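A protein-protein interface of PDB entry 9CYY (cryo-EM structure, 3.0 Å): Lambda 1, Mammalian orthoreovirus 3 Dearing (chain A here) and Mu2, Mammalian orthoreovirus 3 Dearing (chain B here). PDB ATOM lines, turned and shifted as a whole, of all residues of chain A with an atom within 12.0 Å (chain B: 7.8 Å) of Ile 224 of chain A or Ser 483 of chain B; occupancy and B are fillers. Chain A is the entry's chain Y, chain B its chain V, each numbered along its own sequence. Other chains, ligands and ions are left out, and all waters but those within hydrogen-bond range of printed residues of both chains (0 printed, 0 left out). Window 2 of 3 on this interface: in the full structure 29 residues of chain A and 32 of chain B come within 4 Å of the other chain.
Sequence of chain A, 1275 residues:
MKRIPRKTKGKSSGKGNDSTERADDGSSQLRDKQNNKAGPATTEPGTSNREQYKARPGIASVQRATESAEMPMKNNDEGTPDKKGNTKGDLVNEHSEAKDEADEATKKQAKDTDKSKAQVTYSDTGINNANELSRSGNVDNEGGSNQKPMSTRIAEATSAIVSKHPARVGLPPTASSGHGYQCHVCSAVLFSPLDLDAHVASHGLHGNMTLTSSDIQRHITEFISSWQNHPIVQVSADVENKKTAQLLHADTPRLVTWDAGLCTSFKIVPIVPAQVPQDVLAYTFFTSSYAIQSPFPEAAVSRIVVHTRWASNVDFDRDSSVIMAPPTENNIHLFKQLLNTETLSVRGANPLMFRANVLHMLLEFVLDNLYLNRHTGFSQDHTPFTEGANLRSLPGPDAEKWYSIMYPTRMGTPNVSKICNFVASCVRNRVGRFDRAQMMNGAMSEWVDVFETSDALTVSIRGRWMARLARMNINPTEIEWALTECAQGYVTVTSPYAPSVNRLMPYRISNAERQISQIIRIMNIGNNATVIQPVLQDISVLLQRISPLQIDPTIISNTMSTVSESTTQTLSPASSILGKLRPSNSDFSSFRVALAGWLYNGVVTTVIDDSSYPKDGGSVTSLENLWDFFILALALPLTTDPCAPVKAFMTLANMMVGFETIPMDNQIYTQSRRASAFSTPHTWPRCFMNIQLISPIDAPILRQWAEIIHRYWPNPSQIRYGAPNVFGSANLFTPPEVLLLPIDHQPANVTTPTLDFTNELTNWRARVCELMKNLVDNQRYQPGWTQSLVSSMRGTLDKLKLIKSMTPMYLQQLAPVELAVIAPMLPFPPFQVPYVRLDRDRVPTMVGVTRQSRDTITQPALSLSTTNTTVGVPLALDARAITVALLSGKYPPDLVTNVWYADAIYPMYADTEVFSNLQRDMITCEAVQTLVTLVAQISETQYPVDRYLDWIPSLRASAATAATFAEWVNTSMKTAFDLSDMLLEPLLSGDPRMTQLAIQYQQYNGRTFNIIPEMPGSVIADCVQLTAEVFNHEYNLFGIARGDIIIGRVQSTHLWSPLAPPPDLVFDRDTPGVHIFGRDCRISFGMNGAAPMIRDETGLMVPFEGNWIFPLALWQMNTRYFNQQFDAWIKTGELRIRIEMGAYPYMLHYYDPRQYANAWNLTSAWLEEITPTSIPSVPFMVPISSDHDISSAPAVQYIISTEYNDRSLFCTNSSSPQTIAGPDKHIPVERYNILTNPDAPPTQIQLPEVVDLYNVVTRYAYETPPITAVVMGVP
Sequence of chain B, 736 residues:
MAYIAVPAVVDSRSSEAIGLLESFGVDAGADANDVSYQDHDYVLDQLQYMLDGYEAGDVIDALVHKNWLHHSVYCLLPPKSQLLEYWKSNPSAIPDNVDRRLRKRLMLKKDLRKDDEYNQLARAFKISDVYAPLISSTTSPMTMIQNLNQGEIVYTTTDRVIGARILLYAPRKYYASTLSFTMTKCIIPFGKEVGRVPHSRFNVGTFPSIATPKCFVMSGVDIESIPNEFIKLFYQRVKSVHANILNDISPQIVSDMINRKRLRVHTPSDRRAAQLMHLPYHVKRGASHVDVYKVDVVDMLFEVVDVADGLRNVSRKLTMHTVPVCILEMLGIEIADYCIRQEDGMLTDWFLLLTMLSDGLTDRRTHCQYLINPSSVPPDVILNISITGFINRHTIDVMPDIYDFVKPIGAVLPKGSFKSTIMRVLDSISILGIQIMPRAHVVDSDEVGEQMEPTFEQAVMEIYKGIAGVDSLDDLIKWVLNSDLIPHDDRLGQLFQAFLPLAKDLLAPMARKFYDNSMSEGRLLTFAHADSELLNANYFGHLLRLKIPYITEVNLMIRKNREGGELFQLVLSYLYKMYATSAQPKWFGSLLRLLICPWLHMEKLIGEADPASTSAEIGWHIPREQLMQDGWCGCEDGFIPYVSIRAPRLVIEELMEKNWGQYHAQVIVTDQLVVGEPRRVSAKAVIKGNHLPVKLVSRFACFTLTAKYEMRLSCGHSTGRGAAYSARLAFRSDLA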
ATOM      1  N   GLU A 222     -26.865  21.013 -11.518  1.00  0.00           N
ATOM      2  CA  GLU A 222     -26.780  22.460 -11.682  1.00  0.00           C
ATOM      3  C   GLU A 222     -26.849  22.857 -13.150  1.00  0.00           C
ATOM      4  O   GLU A 222     -25.823  22.898 -13.829  1.00  0.00           O
ATOM      5  CB  GLU A 222     -25.491  22.998 -11.058  1.00  0.00           C
ATOM      6  CG  GLU A 222     -25.438  22.892  -9.544  1.00  0.00           C
ATOM      7  CD  GLU A 222     -26.464  23.774  -8.863  1.00  0.00           C
ATOM      8  OE1 GLU A 222     -26.803  24.837  -9.425  1.00  0.00           O
ATOM      9  OE2 GLU A 222     -26.931  23.406  -7.764  1.00  0.00           O
ATOM     10  N   PHE A 223     -28.067  23.155 -13.616  1.00  0.00           N
ATOM     11  CA  PHE A 223     -28.360  23.571 -14.988  1.00  0.00           C
ATOM     12  C   PHE A 223     -27.521  22.819 -16.013  1.00  0.00           C
ATOM     13  O   PHE A 223     -26.934  23.428 -16.913  1.00  0.00           O
ATOM     14  CB  PHE A 223     -28.180  25.089 -15.151  1.00  0.00           C
ATOM     15  CG  PHE A 223     -26.898  25.632 -14.573  1.00  0.00           C
ATOM     16  CD1 PHE A 223     -25.719  25.606 -15.302  1.00  0.00           C
ATOM     17  CD2 PHE A 223     -26.877  26.181 -13.301  1.00  0.00           C
ATOM     18  CE1 PHE A 223     -24.546  26.105 -14.771  1.00  0.00           C
ATOM     19  CE2 PHE A 223     -25.705  26.683 -12.766  1.00  0.00           C
ATOM     20  CZ  PHE A 223     -24.539  26.645 -13.502  1.00  0.00           C
ATOM     21  N   ILE A 224     -27.469  21.491 -15.889  1.00  0.00           N
ATOM     22  CA  ILE A 224     -26.605  20.694 -16.756  1.00  0.00           C
ATOM     23  C   ILE A 224     -27.011  20.860 -18.216  1.00  0.00           C
ATOM     24  O   ILE A 224     -26.158  20.983 -19.103  1.00  0.00           O
ATOM     25  CB  ILE A 224     -26.613  19.216 -16.317  1.00  0.00           C
ATOM     26  CG1 ILE A 224     -25.616  18.405 -17.147  1.00  0.00           C
ATOM     27  CG2 ILE A 224     -28.018  18.620 -16.374  1.00  0.00           C
ATOM     28  CD1 ILE A 224     -24.174  18.793 -16.914  1.00  0.00           C
ATOM     29  N   SER A 225     -28.315  20.861 -18.488  1.00  0.00           N
ATOM     30  CA  SER A 225     -28.886  21.074 -19.815  1.00  0.00           C
ATOM     31  C   SER A 225     -28.389  20.068 -20.845  1.00  0.00           C
ATOM     32  O   SER A 225     -28.646  20.237 -22.043  1.00  0.00           O
ATOM     33  CB  SER A 225     -28.624  22.501 -20.314  1.00  0.00           C
ATOM     34  OG  SER A 225     -28.938  22.623 -21.689  1.00  0.00           O
ATOM     35  N   SER A 226     -27.685  19.022 -20.414  1.00  0.00           N
ATOM     36  CA  SER A 226     -27.117  18.031 -21.317  1.00  0.00           C
ATOM     37  C   SER A 226     -27.779  16.669 -21.214  1.00  0.00           C
ATOM     38  O   SER A 226     -27.758  15.915 -22.188  1.00  0.00           O
ATOM     39  CB  SER A 226     -25.615  17.873 -21.055  1.00  0.00           C
ATOM     40  OG  SER A 226     -24.920  19.072 -21.343  1.00  0.00           O
ATOM     41  N   TRP A 227     -28.355  16.333 -20.059  1.00  0.00           N
ATOM     42  CA  TRP A 227     -29.063  15.064 -19.938  1.00  0.00           C
ATOM     43  C   TRP A 227     -30.294  15.036 -20.832  1.00  0.00           C
ATOM     44  O   TRP A 227     -30.683  13.976 -21.335  1.00  0.00           O
ATOM     45  CB  TRP A 227     -29.455  14.806 -18.486  1.00  0.00           C
ATOM     46  CG  TRP A 227     -30.029  13.446 -18.298  1.00  0.00           C
ATOM     47  CD1 TRP A 227     -29.340  12.275 -18.191  1.00  0.00           C
ATOM     48  CD2 TRP A 227     -31.415  13.105 -18.240  1.00  0.00           C
ATOM     49  NE1 TRP A 227     -30.214  11.226 -18.047  1.00  0.00           N
ATOM     50  CE2 TRP A 227     -31.494  11.709 -18.075  1.00  0.00           C
ATOM     51  CE3 TRP A 227     -32.598  13.845 -18.300  1.00  0.00           C
ATOM     52  CZ2 TRP A 227     -32.709  11.039 -17.971  1.00  0.00           C
ATOM     53  CZ3 TRP A 227     -33.800  13.179 -18.196  1.00  0.00           C
ATOM     54  CH2 TRP A 227     -33.848  11.790 -18.037  1.00  0.00           C
ATOM     55  N   GLN A 228     -30.926  16.194 -21.036  1.00  0.00           N
ATOM     56  CA  GLN A 228     -32.055  16.275 -21.953  1.00  0.00           C
ATOM     57  C   GLN A 228     -31.654  15.933 -23.380  1.00  0.00           C
ATOM     58  O   GLN A 228     -32.520  15.596 -24.194  1.00  0.00           O
ATOM     59  CB  GLN A 228     -32.672  17.675 -21.914  1.00  0.00           C
ATOM     60  CG  GLN A 228     -33.316  18.048 -20.589  1.00  0.00           C
ATOM     61  CD  GLN A 228     -32.303  18.469 -19.542  1.00  0.00           C
ATOM     62  OE1 GLN A 228     -31.135  18.706 -19.852  1.00  0.00           O
ATOM     63  NE2 GLN A 228     -32.745  18.567 -18.295  1.00  0.00           N
ATOM     64  N   ASN A 229     -30.362  16.009 -23.698  1.00  0.00           N
ATOM     65  CA  ASN A 229     -29.880  15.700 -25.036  1.00  0.00           C
ATOM     66  C   ASN A 229     -29.598  14.211 -25.186  1.00  0.00           C
ATOM     67  O   ASN A 229     -28.462  13.816 -25.461  1.00  0.00           O
ATOM     68  CB  ASN A 229     -28.620  16.506 -25.349  1.00  0.00           C
ATOM     69  CG  ASN A 229     -28.840  17.999 -25.228  1.00  0.00           C
ATOM     70  OD1 ASN A 229     -28.266  18.652 -24.358  1.00  0.00           O
ATOM     71  ND2 ASN A 229     -29.677  18.546 -26.100  1.00  0.00           N
ATOM     72  N   HIS A 230     -30.620  13.376 -25.000  1.00  0.00           N
ATOM     73  CA  HIS A 230     -30.473  11.952 -25.246  1.00  0.00           C
ATOM     74  C   HIS A 230     -31.038  11.629 -26.620  1.00  0.00           C
ATOM     75  O   HIS A 230     -32.257  11.740 -26.823  1.00  0.00           O
ATOM     76  CB  HIS A 230     -31.174  11.129 -24.162  1.00  0.00           C
ATOM     77  CG  HIS A 230     -32.621  11.465 -23.975  1.00  0.00           C
ATOM     78  ND1 HIS A 230     -33.042  12.584 -23.290  1.00  0.00           N
ATOM     79  CD2 HIS A 230     -33.744  10.819 -24.366  1.00  0.00           C
ATOM     80  CE1 HIS A 230     -34.363  12.619 -23.278  1.00  0.00           C
ATOM     81  NE2 HIS A 230     -34.813  11.559 -23.924  1.00  0.00           N
ATOM     82  N   LEU A 344     -27.731  22.186 -31.365  1.00  0.00           N
ATOM     83  CA  LEU A 344     -28.414  22.475 -30.109  1.00  0.00           C
ATOM     84  C   LEU A 344     -29.492  23.535 -30.297  1.00  0.00           C
ATOM     85  O   LEU A 344     -30.596  23.417 -29.752  1.00  0.00           O
ATOM     86  CB  LEU A 344     -27.400  22.920 -29.056  1.00  0.00           C
ATOM     87  CG  LEU A 344     -27.958  23.199 -27.661  1.00  0.00           C
ATOM     88  CD1 LEU A 344     -28.558  21.938 -27.065  1.00  0.00           C
ATOM     89  CD2 LEU A 344     -26.876  23.763 -26.756  1.00  0.00           C
ATOM     90  N   VAL B 377     -35.884  24.269 -18.972  1.00  0.00           N
ATOM     91  CA  VAL B 377     -34.475  24.211 -19.376  1.00  0.00           C
ATOM     92  C   VAL B 377     -34.390  24.343 -20.891  1.00  0.00           C
ATOM     93  O   VAL B 377     -35.076  23.591 -21.612  1.00  0.00           O
ATOM     94  CB  VAL B 377     -33.831  22.900 -18.892  1.00  0.00           C
ATOM     95  CG1 VAL B 377     -32.445  22.720 -19.481  1.00  0.00           C
ATOM     96  CG2 VAL B 377     -33.771  22.874 -17.372  1.00  0.00           C
ATOM     97  N   PRO B 379     -33.184  23.521 -23.811  1.00  0.00           N
ATOM     98  CA  PRO B 379     -33.398  22.494 -24.847  1.00  0.00           C
ATOM     99  C   PRO B 379     -34.835  21.994 -24.881  1.00  0.00           C
ATOM    100  O   PRO B 379     -35.334  21.412 -23.914  1.00  0.00           O
ATOM    101  CB  PRO B 379     -32.420  21.382 -24.449  1.00  0.00           C
ATOM    102  CG  PRO B 379     -31.359  22.071 -23.717  1.00  0.00           C
ATOM    103  CD  PRO B 379     -32.036  23.162 -22.954  1.00  0.00           C
ATOM    104  N   LYS B 478     -21.394  10.748  -6.959  1.00  0.00           N
ATOM    105  CA  LYS B 478     -20.410  11.149  -7.961  1.00  0.00           C
ATOM    106  C   LYS B 478     -19.796   9.934  -8.648  1.00  0.00           C
ATOM    107  O   LYS B 478     -19.550   9.954  -9.860  1.00  0.00           O
ATOM    108  CB  LYS B 478     -19.326  12.009  -7.313  1.00  0.00           C
ATOM    109  CG  LYS B 478     -19.832  13.349  -6.806  1.00  0.00           C
ATOM    110  CD  LYS B 478     -18.721  14.160  -6.161  1.00  0.00           C
ATOM    111  CE  LYS B 478     -19.247  15.484  -5.631  1.00  0.00           C
ATOM    112  NZ  LYS B 478     -18.175  16.296  -4.994  1.00  0.00           N
ATOM    113  N   VAL B 480     -21.232   6.812  -8.945  1.00  0.00           N
ATOM    114  CA  VAL B 480     -22.188   6.008  -9.702  1.00  0.00           C
ATOM    115  C   VAL B 480     -22.628   6.741 -10.965  1.00  0.00           C
ATOM    116  O   VAL B 480     -22.828   6.123 -12.018  1.00  0.00           O
ATOM    117  CB  VAL B 480     -23.387   5.611  -8.820  1.00  0.00           C
ATOM    118  CG1 VAL B 480     -24.156   6.832  -8.347  1.00  0.00           C
ATOM    119  CG2 VAL B 480     -24.304   4.655  -9.569  1.00  0.00           C
ATOM    120  N   LEU B 481     -22.783   8.059 -10.889  1.00  0.00           N
ATOM    121  CA  LEU B 481     -23.301   8.803 -12.027  1.00  0.00           C
ATOM    122  C   LEU B 481     -22.174   9.369 -12.883  1.00  0.00           C
ATOM    123  O   LEU B 481     -21.073   9.650 -12.400  1.00  0.00           O
ATOM    124  CB  LEU B 481     -24.220   9.932 -11.560  1.00  0.00           C
ATOM    125  CG  LEU B 481     -25.517   9.461 -10.903  1.00  0.00           C
ATOM    126  CD1 LEU B 481     -26.296  10.636 -10.350  1.00  0.00           C
ATOM    127  CD2 LEU B 481     -26.361   8.682 -11.898  1.00  0.00           C
ATOM    128  N   ASN B 482     -22.468   9.532 -14.170  1.00  0.00           N
ATOM    129  CA  ASN B 482     -21.519  10.072 -15.129  1.00  0.00           C
ATOM    130  C   ASN B 482     -21.577  11.599 -15.117  1.00  0.00           C
ATOM    131  O   ASN B 482     -22.408  12.214 -14.446  1.00  0.00           O
ATOM    132  CB  ASN B 482     -21.813   9.517 -16.522  1.00  0.00           C
ATOM    133  CG  ASN B 482     -20.634   9.639 -17.465  1.00  0.00           C
ATOM    134  OD1 ASN B 482     -19.802  10.535 -17.326  1.00  0.00           O
ATOM    135  ND2 ASN B 482     -20.559   8.735 -18.434  1.00  0.00           N
ATOM    136  N   SER B 483     -20.670  12.223 -15.875  1.00  0.00           N
ATOM    137  CA  SER B 483     -20.693  13.673 -16.019  1.00  0.00           C
ATOM    138  C   SER B 483     -21.940  14.156 -16.745  1.00  0.00           C
ATOM    139  O   SER B 483     -22.296  15.334 -16.628  1.00  0.00           O
ATOM    140  CB  SER B 483     -19.442  14.147 -16.761  1.00  0.00           C
ATOM    141  OG  SER B 483     -19.166  13.312 -17.873  1.00  0.00           O
ATOM    142  N   ASP B 484     -22.609  13.276 -17.489  1.00  0.00           N
ATOM    143  CA  ASP B 484     -23.832  13.605 -18.209  1.00  0.00           C
ATOM    144  C   ASP B 484     -25.077  13.158 -17.445  1.00  0.00           C
ATOM    145  O   ASP B 484     -26.173  13.101 -18.013  1.00  0.00           O
ATOM    146  CB  ASP B 484     -23.795  12.985 -19.607  1.00  0.00           C
ATOM    147  CG  ASP B 484     -24.865  13.543 -20.526  1.00  0.00           C
ATOM    148  OD1 ASP B 484     -24.719  14.701 -20.975  1.00  0.00           O
ATOM    149  OD2 ASP B 484     -25.847  12.825 -20.804  1.00  0.00           O
ATOM    150  N   LEU B 485     -24.918  12.833 -16.160  1.00  0.00           N
ATOM    151  CA  LEU B 485     -26.023  12.407 -15.300  1.00  0.00           C
ATOM    152  C   LEU B 485     -26.678  11.134 -15.829  1.00  0.00           C
ATOM    153  O   LEU B 485     -27.903  11.008 -15.874  1.00  0.00           O
ATOM    154  CB  LEU B 485     -27.055  13.525 -15.132  1.00  0.00           C
ATOM    155  CG  LEU B 485     -26.887  14.442 -13.919  1.00  0.00           C
ATOM    156  CD1 LEU B 485     -25.616  15.267 -14.034  1.00  0.00           C
ATOM    157  CD2 LEU B 485     -28.098  15.344 -13.763  1.00  0.00           C
ATOM    158  N   ILE B 486     -25.850  10.174 -16.229  1.00  0.00           N
ATOM    159  CA  ILE B 486     -26.328   8.883 -16.715  1.00  0.00           C
ATOM    160  C   ILE B 486     -25.619   7.780 -15.935  1.00  0.00           C
ATOM    161  O   ILE B 486     -24.401   7.860 -15.721  1.00  0.00           O
ATOM    162  CB  ILE B 486     -26.106   8.741 -18.229  1.00  0.00           C
ATOM    163  CG1 ILE B 486     -27.029   9.695 -18.991  1.00  0.00           C
ATOM    164  CG2 ILE B 486     -26.332   7.308 -18.685  1.00  0.00           C
ATOM    165  CD1 ILE B 486     -26.796   9.704 -20.482  1.00  0.00           C
ATOM    166  N   HIS B 488     -23.577   4.573 -14.859  1.00  0.00           N
ATOM    167  CA  HIS B 488     -22.740   3.508 -15.474  1.00  0.00           C
ATOM    168  C   HIS B 488     -23.404   2.171 -15.152  1.00  0.00           C
ATOM    169  O   HIS B 488     -23.768   1.970 -13.978  1.00  0.00           O
ATOM    170  CB  HIS B 488     -21.297   3.578 -14.963  1.00  0.00           C
ATOM    171  CG  HIS B 488     -20.895   4.924 -14.462  1.00  0.00           C
ATOM    172  ND1 HIS B 488     -20.996   6.061 -15.238  1.00  0.00           N
ATOM    173  CD2 HIS B 488     -20.386   5.318 -13.276  1.00  0.00           C
ATOM    174  CE1 HIS B 488     -20.568   7.099 -14.548  1.00  0.00           C
ATOM    175  NE2 HIS B 488     -20.190   6.670 -13.340  1.00  0.00           N
ATOM    176  N   MET B 557     -34.918  16.148 -11.048  1.00  0.00           N
ATOM    177  CA  MET B 557     -33.753  17.027 -11.036  1.00  0.00           C
ATOM    178  C   MET B 557     -34.131  18.465 -10.690  1.00  0.00           C
ATOM    179  O   MET B 557     -33.367  19.164 -10.014  1.00  0.00           O
ATOM    180  CB  MET B 557     -33.036  16.970 -12.384  1.00  0.00           C
ATOM    181  CG  MET B 557     -32.484  15.598 -12.732  1.00  0.00           C
ATOM    182  SD  MET B 557     -32.314  15.343 -14.509  1.00  0.00           S
ATOM    183  CE  MET B 557     -31.654  16.929 -15.014  1.00  0.00           C
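The indole nitrogen (NE1) of Trp 227 of chain A sits close to the backbone carbonyl oxygen (O) of Leu 485 of chain B (3.2 Å). O of Ser 226 of chain A sits close to OD1 of Asp 484 of chain B (3.5 Å).
The backbone carbonyl oxygen (O) of Ile 224 of chain A sits at hydrogen-bond distance from the side-chain hydroxyl (OG) of Ser 226 of chain A, 3.2 Å away. O of Ser 225 of chain A sits close to OD1 of Asn 229 of chain A (2.8 Å). The backbone carbonyl oxygen (O) of Trp 227 of chain A is in hydrogen-bond range of a ring nitrogen (ND1) of His 230 of chain A (3.4 Å). A ring nitrogen (ND1) of His 230 of chain A is in hydrogen-bond range of the backbone carbonyl oxygen of Gln 228 of chain A (3.2 Å). The side-chain amide oxygen (OD1) of Asn 482 of chain B lies within hydrogen-bond range of the side-chain hydroxyl (OG) of Ser 483 of chain B (2.9 Å).
Among the printed residues, merely in contact across the chains: Ile 224 of chain A with Ser 483 of chain B, Ser 225 of chain A with Val 377 of chain B, Ser 225 of chain A with Pro 379 of chain B, Trp 227 of chain A with Asp 484 of chain B, Trp 227 of chain A with Ile 486 of chain B and Gln 228 of chain A with Met 557 of chain B.
Printed residues of chain B within 4 Å of Gln 228 of chain A: Met 557 (3.8 Å). Of the printed residues of chain A, Val 377 of chain B touches Ser 225 (3.9 Å). Val 480 of chain B touches none of the printed residues of chain A. Of chain A, only Ile 224 comes within 4 Å of Ser 483 of chain B. Asp 484 of chain B touches just these residues of chain A: Ser 226 and Trp 227. Of chain A, only Trp 227 (3.0 Å) comes within 4 Å of Leu 485 of chain B.
Of the 12 printed residues of chain B, 7 touch a printed residue of chain A. Printed residues of chain B that touch a printed residue of chain A: Val 377, Pro 379, Ser 483, Asp 484, Leu 485, Ile 486 and Met 557.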
